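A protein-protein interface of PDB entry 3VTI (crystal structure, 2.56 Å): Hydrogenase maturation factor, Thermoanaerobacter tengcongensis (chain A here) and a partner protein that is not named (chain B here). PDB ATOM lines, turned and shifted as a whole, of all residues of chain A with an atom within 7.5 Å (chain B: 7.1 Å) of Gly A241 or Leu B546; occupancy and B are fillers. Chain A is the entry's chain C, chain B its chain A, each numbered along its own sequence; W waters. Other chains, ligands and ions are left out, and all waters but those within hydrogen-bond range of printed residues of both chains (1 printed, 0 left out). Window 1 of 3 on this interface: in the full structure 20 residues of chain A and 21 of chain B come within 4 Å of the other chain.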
ATOM      1  N   SER A 235      -9.253 -18.354 -30.470  1.00  0.00           N
ATOM      2  CA  SER A 235      -9.016 -19.787 -30.284  1.00  0.00           C
ATOM      3  C   SER A 235      -7.665 -20.273 -30.837  1.00  0.00           C
ATOM      4  O   SER A 235      -7.116 -21.254 -30.341  1.00  0.00           O
ATOM      5  CB  SER A 235     -10.187 -20.624 -30.819  1.00  0.00           C
ATOM      6  OG  SER A 235     -10.279 -20.559 -32.220  1.00  0.00           O
ATOM      7  N   ALA A 236      -7.134 -19.587 -31.848  1.00  0.00           N
ATOM      8  CA  ALA A 236      -5.797 -19.882 -32.351  1.00  0.00           C
ATOM      9  C   ALA A 236      -4.758 -19.667 -31.247  1.00  0.00           C
ATOM     10  O   ALA A 236      -3.880 -20.519 -31.026  1.00  0.00           O
ATOM     11  CB  ALA A 236      -5.481 -19.026 -33.555  1.00  0.00           C
ATOM     12  N   CYS A 237      -4.875 -18.527 -30.561  1.00  0.00           N
ATOM     13  CA  CYS A 237      -4.039 -18.186 -29.416  1.00  0.00           C
ATOM     14  C   CYS A 237      -4.303 -19.109 -28.223  1.00  0.00           C
ATOM     15  O   CYS A 237      -3.374 -19.478 -27.512  1.00  0.00           O
ATOM     16  CB  CYS A 237      -4.273 -16.727 -29.000  1.00  0.00           C
ATOM     17  SG  CYS A 237      -3.715 -15.463 -30.192  1.00  0.00           S
ATOM     18  N   GLU A 238      -5.566 -19.466 -28.005  1.00  0.00           N
ATOM     19  CA  GLU A 238      -5.954 -20.310 -26.876  1.00  0.00           C
ATOM     20  C   GLU A 238      -5.438 -21.738 -27.063  1.00  0.00           C
ATOM     21  O   GLU A 238      -5.259 -22.480 -26.095  1.00  0.00           O
ATOM     22  CB  GLU A 238      -7.475 -20.310 -26.704  1.00  0.00           C
ATOM     23  CG  GLU A 238      -7.946 -20.455 -25.264  1.00  0.00           C
ATOM     24  CD  GLU A 238      -7.900 -21.889 -24.761  1.00  0.00           C
ATOM     25  OE1 GLU A 238      -7.584 -22.089 -23.572  1.00  0.00           O
ATOM     26  OE2 GLU A 238      -8.176 -22.818 -25.552  1.00  0.00           O
ATOM     27  N   PHE A 239      -5.197 -22.117 -28.313  1.00  0.00           N
ATOM     28  CA  PHE A 239      -4.676 -23.436 -28.620  1.00  0.00           C
ATOM     29  C   PHE A 239      -3.185 -23.534 -28.379  1.00  0.00           C
ATOM     30  O   PHE A 239      -2.678 -24.613 -28.118  1.00  0.00           O
ATOM     31  CB  PHE A 239      -4.984 -23.811 -30.063  1.00  0.00           C
ATOM     32  CG  PHE A 239      -6.366 -24.349 -30.266  1.00  0.00           C
ATOM     33  CD1 PHE A 239      -7.108 -24.825 -29.190  1.00  0.00           C
ATOM     34  CD2 PHE A 239      -6.916 -24.405 -31.543  1.00  0.00           C
ATOM     35  CE1 PHE A 239      -8.382 -25.333 -29.375  1.00  0.00           C
ATOM     36  CE2 PHE A 239      -8.187 -24.914 -31.747  1.00  0.00           C
ATOM     37  CZ  PHE A 239      -8.926 -25.382 -30.659  1.00  0.00           C
ATOM     38  N   MET A 240      -2.496 -22.403 -28.472  1.00  0.00           N
ATOM     39  CA  MET A 240      -1.048 -22.356 -28.332  1.00  0.00           C
ATOM     40  C   MET A 240      -0.630 -21.664 -27.046  1.00  0.00           C
ATOM     41  O   MET A 240       0.565 -21.518 -26.782  1.00  0.00           O
ATOM     42  CB  MET A 240      -0.420 -21.623 -29.514  1.00  0.00           C
ATOM     43  CG  MET A 240      -0.626 -22.286 -30.857  1.00  0.00           C
ATOM     44  SD  MET A 240      -0.005 -21.248 -32.182  1.00  0.00           S
ATOM     45  CE  MET A 240       1.746 -21.581 -32.037  1.00  0.00           C
ATOM     46  N   GLY A 241      -1.611 -21.229 -26.259  1.00  0.00           N
ATOM     47  CA  GLY A 241      -1.351 -20.497 -25.019  1.00  0.00           C
ATOM     48  C   GLY A 241      -0.716 -19.123 -25.194  1.00  0.00           C
ATOM     49  O   GLY A 241       0.067 -18.692 -24.347  1.00  0.00           O
ATOM     50  N   ILE A 242      -1.054 -18.443 -26.293  1.00  0.00           N
ATOM     51  CA  ILE A 242      -0.529 -17.118 -26.601  1.00  0.00           C
ATOM     52  C   ILE A 242      -1.484 -16.019 -26.120  1.00  0.00           C
ATOM     53  O   ILE A 242      -2.697 -16.221 -26.075  1.00  0.00           O
ATOM     54  CB  ILE A 242      -0.288 -16.959 -28.125  1.00  0.00           C
ATOM     55  CG1 ILE A 242       0.852 -17.867 -28.578  1.00  0.00           C
ATOM     56  CG2 ILE A 242       0.047 -15.521 -28.493  1.00  0.00           C
ATOM     57  CD1 ILE A 242       0.903 -18.082 -30.089  1.00  0.00           C
ATOM     58  N   ASP A 243      -0.924 -14.866 -25.757  1.00  0.00           N
ATOM     59  CA  ASP A 243      -1.703 -13.671 -25.415  1.00  0.00           C
ATOM     60  C   ASP A 243      -1.776 -12.786 -26.654  1.00  0.00           C
ATOM     61  O   ASP A 243      -0.742 -12.311 -27.131  1.00  0.00           O
ATOM     62  CB  ASP A 243      -1.031 -12.910 -24.259  1.00  0.00           C
ATOM     63  CG  ASP A 243      -1.959 -11.901 -23.582  1.00  0.00           C
ATOM     64  OD1 ASP A 243      -2.851 -11.334 -24.260  1.00  0.00           O
ATOM     65  OD2 ASP A 243      -1.787 -11.664 -22.360  1.00  0.00           O
ATOM     66  N   PHE A 244      -2.978 -12.559 -27.186  1.00  0.00           N
ATOM     67  CA  PHE A 244      -3.114 -11.728 -28.401  1.00  0.00           C
ATOM     68  C   PHE A 244      -2.608 -10.297 -28.229  1.00  0.00           C
ATOM     69  O   PHE A 244      -2.339  -9.589 -29.210  1.00  0.00           O
ATOM     70  CB  PHE A 244      -4.533 -11.755 -28.980  1.00  0.00           C
ATOM     71  CG  PHE A 244      -5.612 -11.415 -27.993  1.00  0.00           C
ATOM     72  CD1 PHE A 244      -5.855 -10.093 -27.631  1.00  0.00           C
ATOM     73  CD2 PHE A 244      -6.406 -12.423 -27.447  1.00  0.00           C
ATOM     74  CE1 PHE A 244      -6.848  -9.773 -26.732  1.00  0.00           C
ATOM     75  CE2 PHE A 244      -7.419 -12.117 -26.541  1.00  0.00           C
ATOM     76  CZ  PHE A 244      -7.639 -10.783 -26.184  1.00  0.00           C
ATOM     77  N   LEU B 541       7.105 -27.670 -22.790  1.00  0.00           N
ATOM     78  CA  LEU B 541       5.855 -27.251 -22.175  1.00  0.00           C
ATOM     79  C   LEU B 541       5.129 -26.356 -23.165  1.00  0.00           C
ATOM     80  O   LEU B 541       5.374 -25.145 -23.208  1.00  0.00           O
ATOM     81  CB  LEU B 541       6.115 -26.494 -20.875  1.00  0.00           C
ATOM     82  CG  LEU B 541       4.918 -26.140 -19.984  1.00  0.00           C
ATOM     83  CD1 LEU B 541       4.436 -27.374 -19.225  1.00  0.00           C
ATOM     84  CD2 LEU B 541       5.282 -25.018 -19.010  1.00  0.00           C
ATOM     85  N   PRO B 542       4.243 -26.954 -23.980  1.00  0.00           N
ATOM     86  CA  PRO B 542       3.562 -26.228 -25.045  1.00  0.00           C
ATOM     87  C   PRO B 542       2.550 -25.246 -24.478  1.00  0.00           C
ATOM     88  O   PRO B 542       1.629 -25.642 -23.760  1.00  0.00           O
ATOM     89  CB  PRO B 542       2.877 -27.337 -25.848  1.00  0.00           C
ATOM     90  CG  PRO B 542       2.698 -28.458 -24.899  1.00  0.00           C
ATOM     91  CD  PRO B 542       3.769 -28.346 -23.855  1.00  0.00           C
ATOM     92  N   GLY B 543       2.742 -23.967 -24.782  1.00  0.00           N
ATOM     93  CA  GLY B 543       1.853 -22.922 -24.295  1.00  0.00           C
ATOM     94  C   GLY B 543       2.249 -22.349 -22.947  1.00  0.00           C
ATOM     95  O   GLY B 543       1.522 -21.525 -22.391  1.00  0.00           O
ATOM     96  N   ASN B 544       3.401 -22.778 -22.431  1.00  0.00           N
ATOM     97  CA  ASN B 544       3.930 -22.295 -21.150  1.00  0.00           C
ATOM     98  C   ASN B 544       2.875 -22.190 -20.047  1.00  0.00           C
ATOM     99  O   ASN B 544       2.429 -23.215 -19.513  1.00  0.00           O
ATOM    100  CB  ASN B 544       4.664 -20.959 -21.315  1.00  0.00           C
ATOM    101  CG  ASN B 544       6.010 -21.112 -21.985  1.00  0.00           C
ATOM    102  OD1 ASN B 544       6.685 -22.134 -21.827  1.00  0.00           O
ATOM    103  ND2 ASN B 544       6.412 -20.095 -22.743  1.00  0.00           N
ATOM    104  N   GLU B 545       2.474 -20.952 -19.732  1.00  0.00           N
ATOM    105  CA  GLU B 545       1.546 -20.671 -18.639  1.00  0.00           C
ATOM    106  C   GLU B 545       0.205 -21.423 -18.755  1.00  0.00           C
ATOM    107  O   GLU B 545      -0.296 -21.953 -17.755  1.00  0.00           O
ATOM    108  CB  GLU B 545       1.339 -19.160 -18.479  1.00  0.00           C
ATOM    109  CG  GLU B 545       0.351 -18.761 -17.387  1.00  0.00           C
ATOM    110  CD  GLU B 545       0.572 -19.511 -16.069  1.00  0.00           C
ATOM    111  OE1 GLU B 545       1.741 -19.608 -15.603  1.00  0.00           O
ATOM    112  OE2 GLU B 545      -0.435 -20.009 -15.503  1.00  0.00           O
ATOM    113  N   LEU B 546      -0.357 -21.481 -19.963  1.00  0.00           N
ATOM    114  CA  LEU B 546      -1.631 -22.167 -20.189  1.00  0.00           C
ATOM    115  C   LEU B 546      -1.570 -23.659 -19.818  1.00  0.00           C
ATOM    116  O   LEU B 546      -2.549 -24.212 -19.302  1.00  0.00           O
ATOM    117  CB  LEU B 546      -2.101 -21.998 -21.636  1.00  0.00           C
ATOM    118  CG  LEU B 546      -3.558 -22.393 -21.943  1.00  0.00           C
ATOM    119  CD1 LEU B 546      -4.535 -21.254 -21.645  1.00  0.00           C
ATOM    120  CD2 LEU B 546      -3.716 -22.851 -23.387  1.00  0.00           C
ATOM    121  N   ALA B 547      -0.420 -24.291 -20.068  1.00  0.00           N
ATOM    122  CA  ALA B 547      -0.236 -25.726 -19.811  1.00  0.00           C
ATOM    123  C   ALA B 547      -0.247 -26.034 -18.322  1.00  0.00           C
ATOM    124  O   ALA B 547      -0.431 -27.181 -17.920  1.00  0.00           O
ATOM    125  CB  ALA B 547       1.056 -26.229 -20.443  1.00  0.00           C
ATOM    126  N   ILE B 548      -0.048 -25.005 -17.508  1.00  0.00           N
ATOM    127  CA  ILE B 548      -0.026 -25.161 -16.066  1.00  0.00           C
ATOM    128  C   ILE B 548      -1.452 -25.142 -15.512  1.00  0.00           C
ATOM    129  O   ILE B 548      -1.722 -25.738 -14.472  1.00  0.00           O
ATOM    130  CB  ILE B 548       0.908 -24.110 -15.392  1.00  0.00           C
ATOM    131  CG1 ILE B 548       2.348 -24.291 -15.907  1.00  0.00           C
ATOM    132  CG2 ILE B 548       0.848 -24.222 -13.878  1.00  0.00           C
ATOM    133  CD1 ILE B 548       3.397 -23.391 -15.259  1.00  0.00           C
ATOM    134  N   LYS B 549      -2.361 -24.463 -16.208  1.00  0.00           N
ATOM    135  CA  LYS B 549      -3.780 -24.532 -15.886  1.00  0.00           C
ATOM    136  C   LYS B 549      -4.376 -25.789 -16.532  1.00  0.00           C
ATOM    137  O   LYS B 549      -4.967 -26.631 -15.854  1.00  0.00           O
ATOM    138  CB  LYS B 549      -4.502 -23.270 -16.368  1.00  0.00           C
ATOM    139  CG  LYS B 549      -5.456 -22.621 -15.344  1.00  0.00           C
ATOM    140  CD  LYS B 549      -4.723 -22.286 -14.004  1.00  0.00           C
ATOM    141  CE  LYS B 549      -5.564 -21.418 -13.059  1.00  0.00           C
ATOM    142  NZ  LYS B 549      -5.664 -19.999 -13.549  1.00  0.00           N
ATOM    143  N   LYS B 550      -4.194 -25.922 -17.843  1.00  0.00           N
ATOM    144  CA  LYS B 550      -4.645 -27.100 -18.580  1.00  0.00           C
ATOM    145  C   LYS B 550      -3.508 -28.119 -18.619  1.00  0.00           C
ATOM    146  O   LYS B 550      -2.692 -28.137 -19.546  1.00  0.00           O
ATOM    147  CB  LYS B 550      -5.106 -26.713 -19.988  1.00  0.00           C
ATOM    148  CG  LYS B 550      -6.261 -25.730 -20.004  1.00  0.00           C
ATOM    149  CD  LYS B 550      -6.744 -25.470 -21.416  1.00  0.00           C
ATOM    150  CE  LYS B 550      -8.036 -24.639 -21.422  1.00  0.00           C
ATOM    151  NZ  LYS B 550      -8.660 -24.583 -22.792  1.00  0.00           N
ATOM    152  N   ILE B 551      -3.466 -28.962 -17.590  1.00  0.00           N
ATOM    153  CA  ILE B 551      -2.326 -29.847 -17.340  1.00  0.00           C
ATOM    154  C   ILE B 551      -2.234 -31.028 -18.307  1.00  0.00           C
ATOM    155  O   ILE B 551      -1.188 -31.655 -18.407  1.00  0.00           O
ATOM    156  CB  ILE B 551      -2.229 -30.296 -15.853  1.00  0.00           C
ATOM    157  CG1 ILE B 551      -3.505 -30.998 -15.397  1.00  0.00           C
ATOM    158  CG2 ILE B 551      -1.963 -29.090 -14.957  1.00  0.00           C
ATOM    159  CD1 ILE B 551      -3.300 -31.926 -14.216  1.00  0.00           C
ATOM    160  N   TYR B 552      -3.312 -31.306 -19.040  1.00  0.00           N
ATOM    161  CA  TYR B 552      -3.245 -32.282 -20.136  1.00  0.00           C
ATOM    162  C   TYR B 552      -2.253 -31.864 -21.231  1.00  0.00           C
ATOM    163  O   TYR B 552      -1.716 -32.712 -21.940  1.00  0.00           O
ATOM    164  CB  TYR B 552      -4.641 -32.610 -20.714  1.00  0.00           C
ATOM    165  CG  TYR B 552      -5.299 -31.511 -21.525  1.00  0.00           C
ATOM    166  CD1 TYR B 552      -6.196 -30.609 -20.929  1.00  0.00           C
ATOM    167  CD2 TYR B 552      -5.043 -31.380 -22.890  1.00  0.00           C
ATOM    168  CE1 TYR B 552      -6.810 -29.594 -21.676  1.00  0.00           C
ATOM    169  CE2 TYR B 552      -5.641 -30.377 -23.637  1.00  0.00           C
ATOM    170  CZ  TYR B 552      -6.523 -29.494 -23.031  1.00  0.00           C
ATOM    171  OH  TYR B 552      -7.110 -28.514 -23.794  1.00  0.00           O
ATOM    172  N   ARG B 553      -2.023 -30.558 -21.354  1.00  0.00           N
ATOM    173  CA  ARG B 553      -1.010 -30.019 -22.262  1.00  0.00           C
ATOM    174  C   ARG B 553       0.404 -30.354 -21.785  1.00  0.00           C
ATOM    175  O   ARG B 553       1.281 -30.664 -22.597  1.00  0.00           O
ATOM    176  CB  ARG B 553      -1.149 -28.507 -22.397  1.00  0.00           C
ATOM    177  CG  ARG B 553      -2.427 -28.036 -23.068  1.00  0.00           C
ATOM    178  CD  ARG B 553      -2.473 -26.514 -23.103  1.00  0.00           C
ATOM    179  NE  ARG B 553      -1.452 -25.959 -23.991  1.00  0.00           N
ATOM    180  CZ  ARG B 553      -1.677 -25.598 -25.253  1.00  0.00           C
ATOM    181  NH1 ARG B 553      -2.893 -25.712 -25.772  1.00  0.00           N
ATOM    182  NH2 ARG B 553      -0.688 -25.115 -25.993  1.00  0.00           N
ATOM    183  N   THR B 554       0.612 -30.274 -20.471  1.00  0.00           N
ATOM    184  CA  THR B 554       1.868 -30.690 -19.839  1.00  0.00           C
ATOM    185  C   THR B 554       2.146 -32.179 -20.112  1.00  0.00           C
ATOM    186  O   THR B 554       3.256 -32.548 -20.520  1.00  0.00           O
ATOM    187  CB  THR B 554       1.851 -30.407 -18.318  1.00  0.00           C
ATOM    188  OG1 THR B 554       1.537 -29.023 -18.096  1.00  0.00           O
ATOM    189  CG2 THR B 554       3.191 -30.733 -17.682  1.00  0.00           C
ATOM    190  N   GLU B 577      -6.778 -29.281 -31.824  1.00  0.00           N
ATOM    191  CA  GLU B 577      -5.910 -28.814 -30.755  1.00  0.00           C
ATOM    192  C   GLU B 577      -4.625 -29.633 -30.700  1.00  0.00           C
ATOM    193  O   GLU B 577      -3.533 -29.069 -30.611  1.00  0.00           O
ATOM    194  CB  GLU B 577      -6.628 -28.841 -29.403  1.00  0.00           C
ATOM    195  CG  GLU B 577      -5.854 -28.106 -28.295  1.00  0.00           C
ATOM    196  CD  GLU B 577      -6.509 -28.186 -26.935  1.00  0.00           C
ATOM    197  OE1 GLU B 577      -7.596 -28.783 -26.815  1.00  0.00           O
ATOM    198  OE2 GLU B 577      -5.928 -27.645 -25.972  1.00  0.00           O
ATOM    199  N   GLN B 584       3.301 -26.728 -32.631  1.00  0.00           N
ATOM    200  CA  GLN B 584       3.972 -25.627 -31.932  1.00  0.00           C
ATOM    201  C   GLN B 584       5.236 -26.094 -31.212  1.00  0.00           C
ATOM    202  O   GLN B 584       6.192 -25.332 -31.075  1.00  0.00           O
ATOM    203  CB  GLN B 584       3.026 -24.864 -30.983  1.00  0.00           C
ATOM    204  CG  GLN B 584       2.753 -25.541 -29.655  1.00  0.00           C
ATOM    205  CD  GLN B 584       1.997 -24.663 -28.677  1.00  0.00           C
ATOM    206  OE1 GLN B 584       2.441 -23.561 -28.330  1.00  0.00           O
ATOM    207  NE2 GLN B 584       0.853 -25.157 -28.212  1.00  0.00           N
ATOM    208  N   ASN B 590       6.175 -20.526 -28.460  1.00  0.00           N
ATOM    209  CA  ASN B 590       5.647 -20.413 -27.105  1.00  0.00           C
ATOM    210  C   ASN B 590       5.777 -21.738 -26.358  1.00  0.00           C
ATOM    211  O   ASN B 590       4.797 -22.285 -25.852  1.00  0.00           O
ATOM    212  CB  ASN B 590       4.197 -19.910 -27.115  1.00  0.00           C
ATOM    213  CG  ASN B 590       3.727 -19.457 -25.746  1.00  0.00           C
ATOM    214  OD1 ASN B 590       4.477 -18.841 -24.994  1.00  0.00           O
ATOM    215  ND2 ASN B 590       2.486 -19.766 -25.411  1.00  0.00           N
ATOM    216  N   GLU B 613      -7.825 -30.203 -16.052  1.00  0.00           N
ATOM    217  CA  GLU B 613      -7.587 -28.778 -15.855  1.00  0.00           C
ATOM    218  C   GLU B 613      -7.687 -28.430 -14.370  1.00  0.00           C
ATOM    219  O   GLU B 613      -8.481 -29.023 -13.646  1.00  0.00           O
ATOM    220  CB  GLU B 613      -8.605 -27.971 -16.660  1.00  0.00           C
ATOM    221  CG  GLU B 613      -8.271 -26.499 -16.803  1.00  0.00           C
ATOM    222  CD  GLU B 613      -9.410 -25.707 -17.399  1.00  0.00           C
ATOM    223  OE1 GLU B 613      -9.878 -26.076 -18.498  1.00  0.00           O
ATOM    224  OE2 GLU B 613      -9.830 -24.712 -16.765  1.00  0.00           O
HETATM  225  O   HOH W   1      -5.389 -25.577 -24.528  1.00  0.00           O
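NZ of Lys B550 is in salt-bridge range of OE1 of Glu A238. The guanidinium group of Arg B553 is in hydrogen-bond range of the backbone carbonyl oxygen of Phe A239 (2.6 Å). The side-chain amide oxygen (OE1) of Gln B584 lies close to the backbone carbonyl oxygen (O) of Met A240 (3.2 Å). The backbone carbonyl oxygen of Met A240 is in hydrogen-bond range of the side-chain amide nitrogen of Asn B590, at 2.9 Å. The side-chain amide nitrogen of Asn B590 is in hydrogen-bond range of the backbone carbonyl oxygen of Gly A241 (2.9 Å).
The backbone carbonyl oxygen (O) of Pro B542 sits at hydrogen-bond distance from the guanidinium group (NE) of Arg B553 (3.1 Å). The backbone NH (N) of Gly B543 lies within hydrogen-bond range of the backbone carbonyl oxygen (O) of Asn B590 (2.9 Å). The side-chain amide nitrogen (ND2) of Asn B544 sits at hydrogen-bond distance from the side-chain amide oxygen (OD1) of Asn B590 (3.2 Å). OE2 of Glu B577 is in hydrogen-bond range of OH of Tyr B552 (2.6 Å). NH2 of Arg B553 sits close to NE2 of Gln B584, at 2.7 Å. The backbone carbonyl oxygen of Cys A237 sits at hydrogen-bond distance from the backbone NH of Ile A242, 2.8 Å away.
Glu A238 touches Leu B546 (O to CD2, 3.1 Å). CD1 of Phe A239 touches CG of Glu B577, 3.6 Å away. NE2 of Gln B584 touches O of Phe A239, at 3.6 Å. Met A240 touches Gly B543 (O to CA, 3.1 Å). C of Met A240 touches NH2 of Arg B553, 3.6 Å away. Gly A241 touches Gly B543. Leu B546 touches Gly A241 (CD2 to CA, 3.7 Å). Ile A242 touches Asn B590 (N to ND2, 3.9 Å).
Cys A237 touches none of the printed residues of chain B. Printed residues of chain B within 4 Å of Phe A239: Arg B553, Glu B577 and Gln B584. Printed residues of chain B within 4 Å of Met A240: Gly B543 (3.1 Å), Arg B553 (3.6 Å), Gln B584 (3.2 Å) and Asn B590 (2.9 Å). Of the printed residues of chain B, Gly A241 touches Gly B543, Leu B546 and Asn B590. Asp A243 touches none of the printed residues of chain B. Of the printed residues of chain A, Gly B543 touches Met A240 (3.1 Å) and Gly A241 (3.7 Å). Leu B546 touches just these residues of chain A: Glu A238 (3.1 Å) and Gly A241 (3.7 Å). Of the printed residues of chain A, Glu B577 touches Phe A239.
Of the 10 printed residues of chain A, 5 touch a printed residue of chain B. Printed residues of chain A that touch a printed residue of chain B: Glu A238, Phe A239, Met A240, Gly A241 and Ile A242. Hydrophobic or aromatic side chains of chain A that line the printed part of chain B: Phe A239 and Met A240. Hydrophobic or aromatic side chains of chain B within 4 Å of the printed part of chain A: Leu B546. Among the printed residues, 13 pairs touch across the chains.
Water W1 lies within hydrogen-bond range of OE2 of Glu B577 (2.6 Å), NH1 of Arg B553 (2.8 Å), O of Glu A238 (3.5 Å) and OH of Tyr B552 (3.5 Å).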
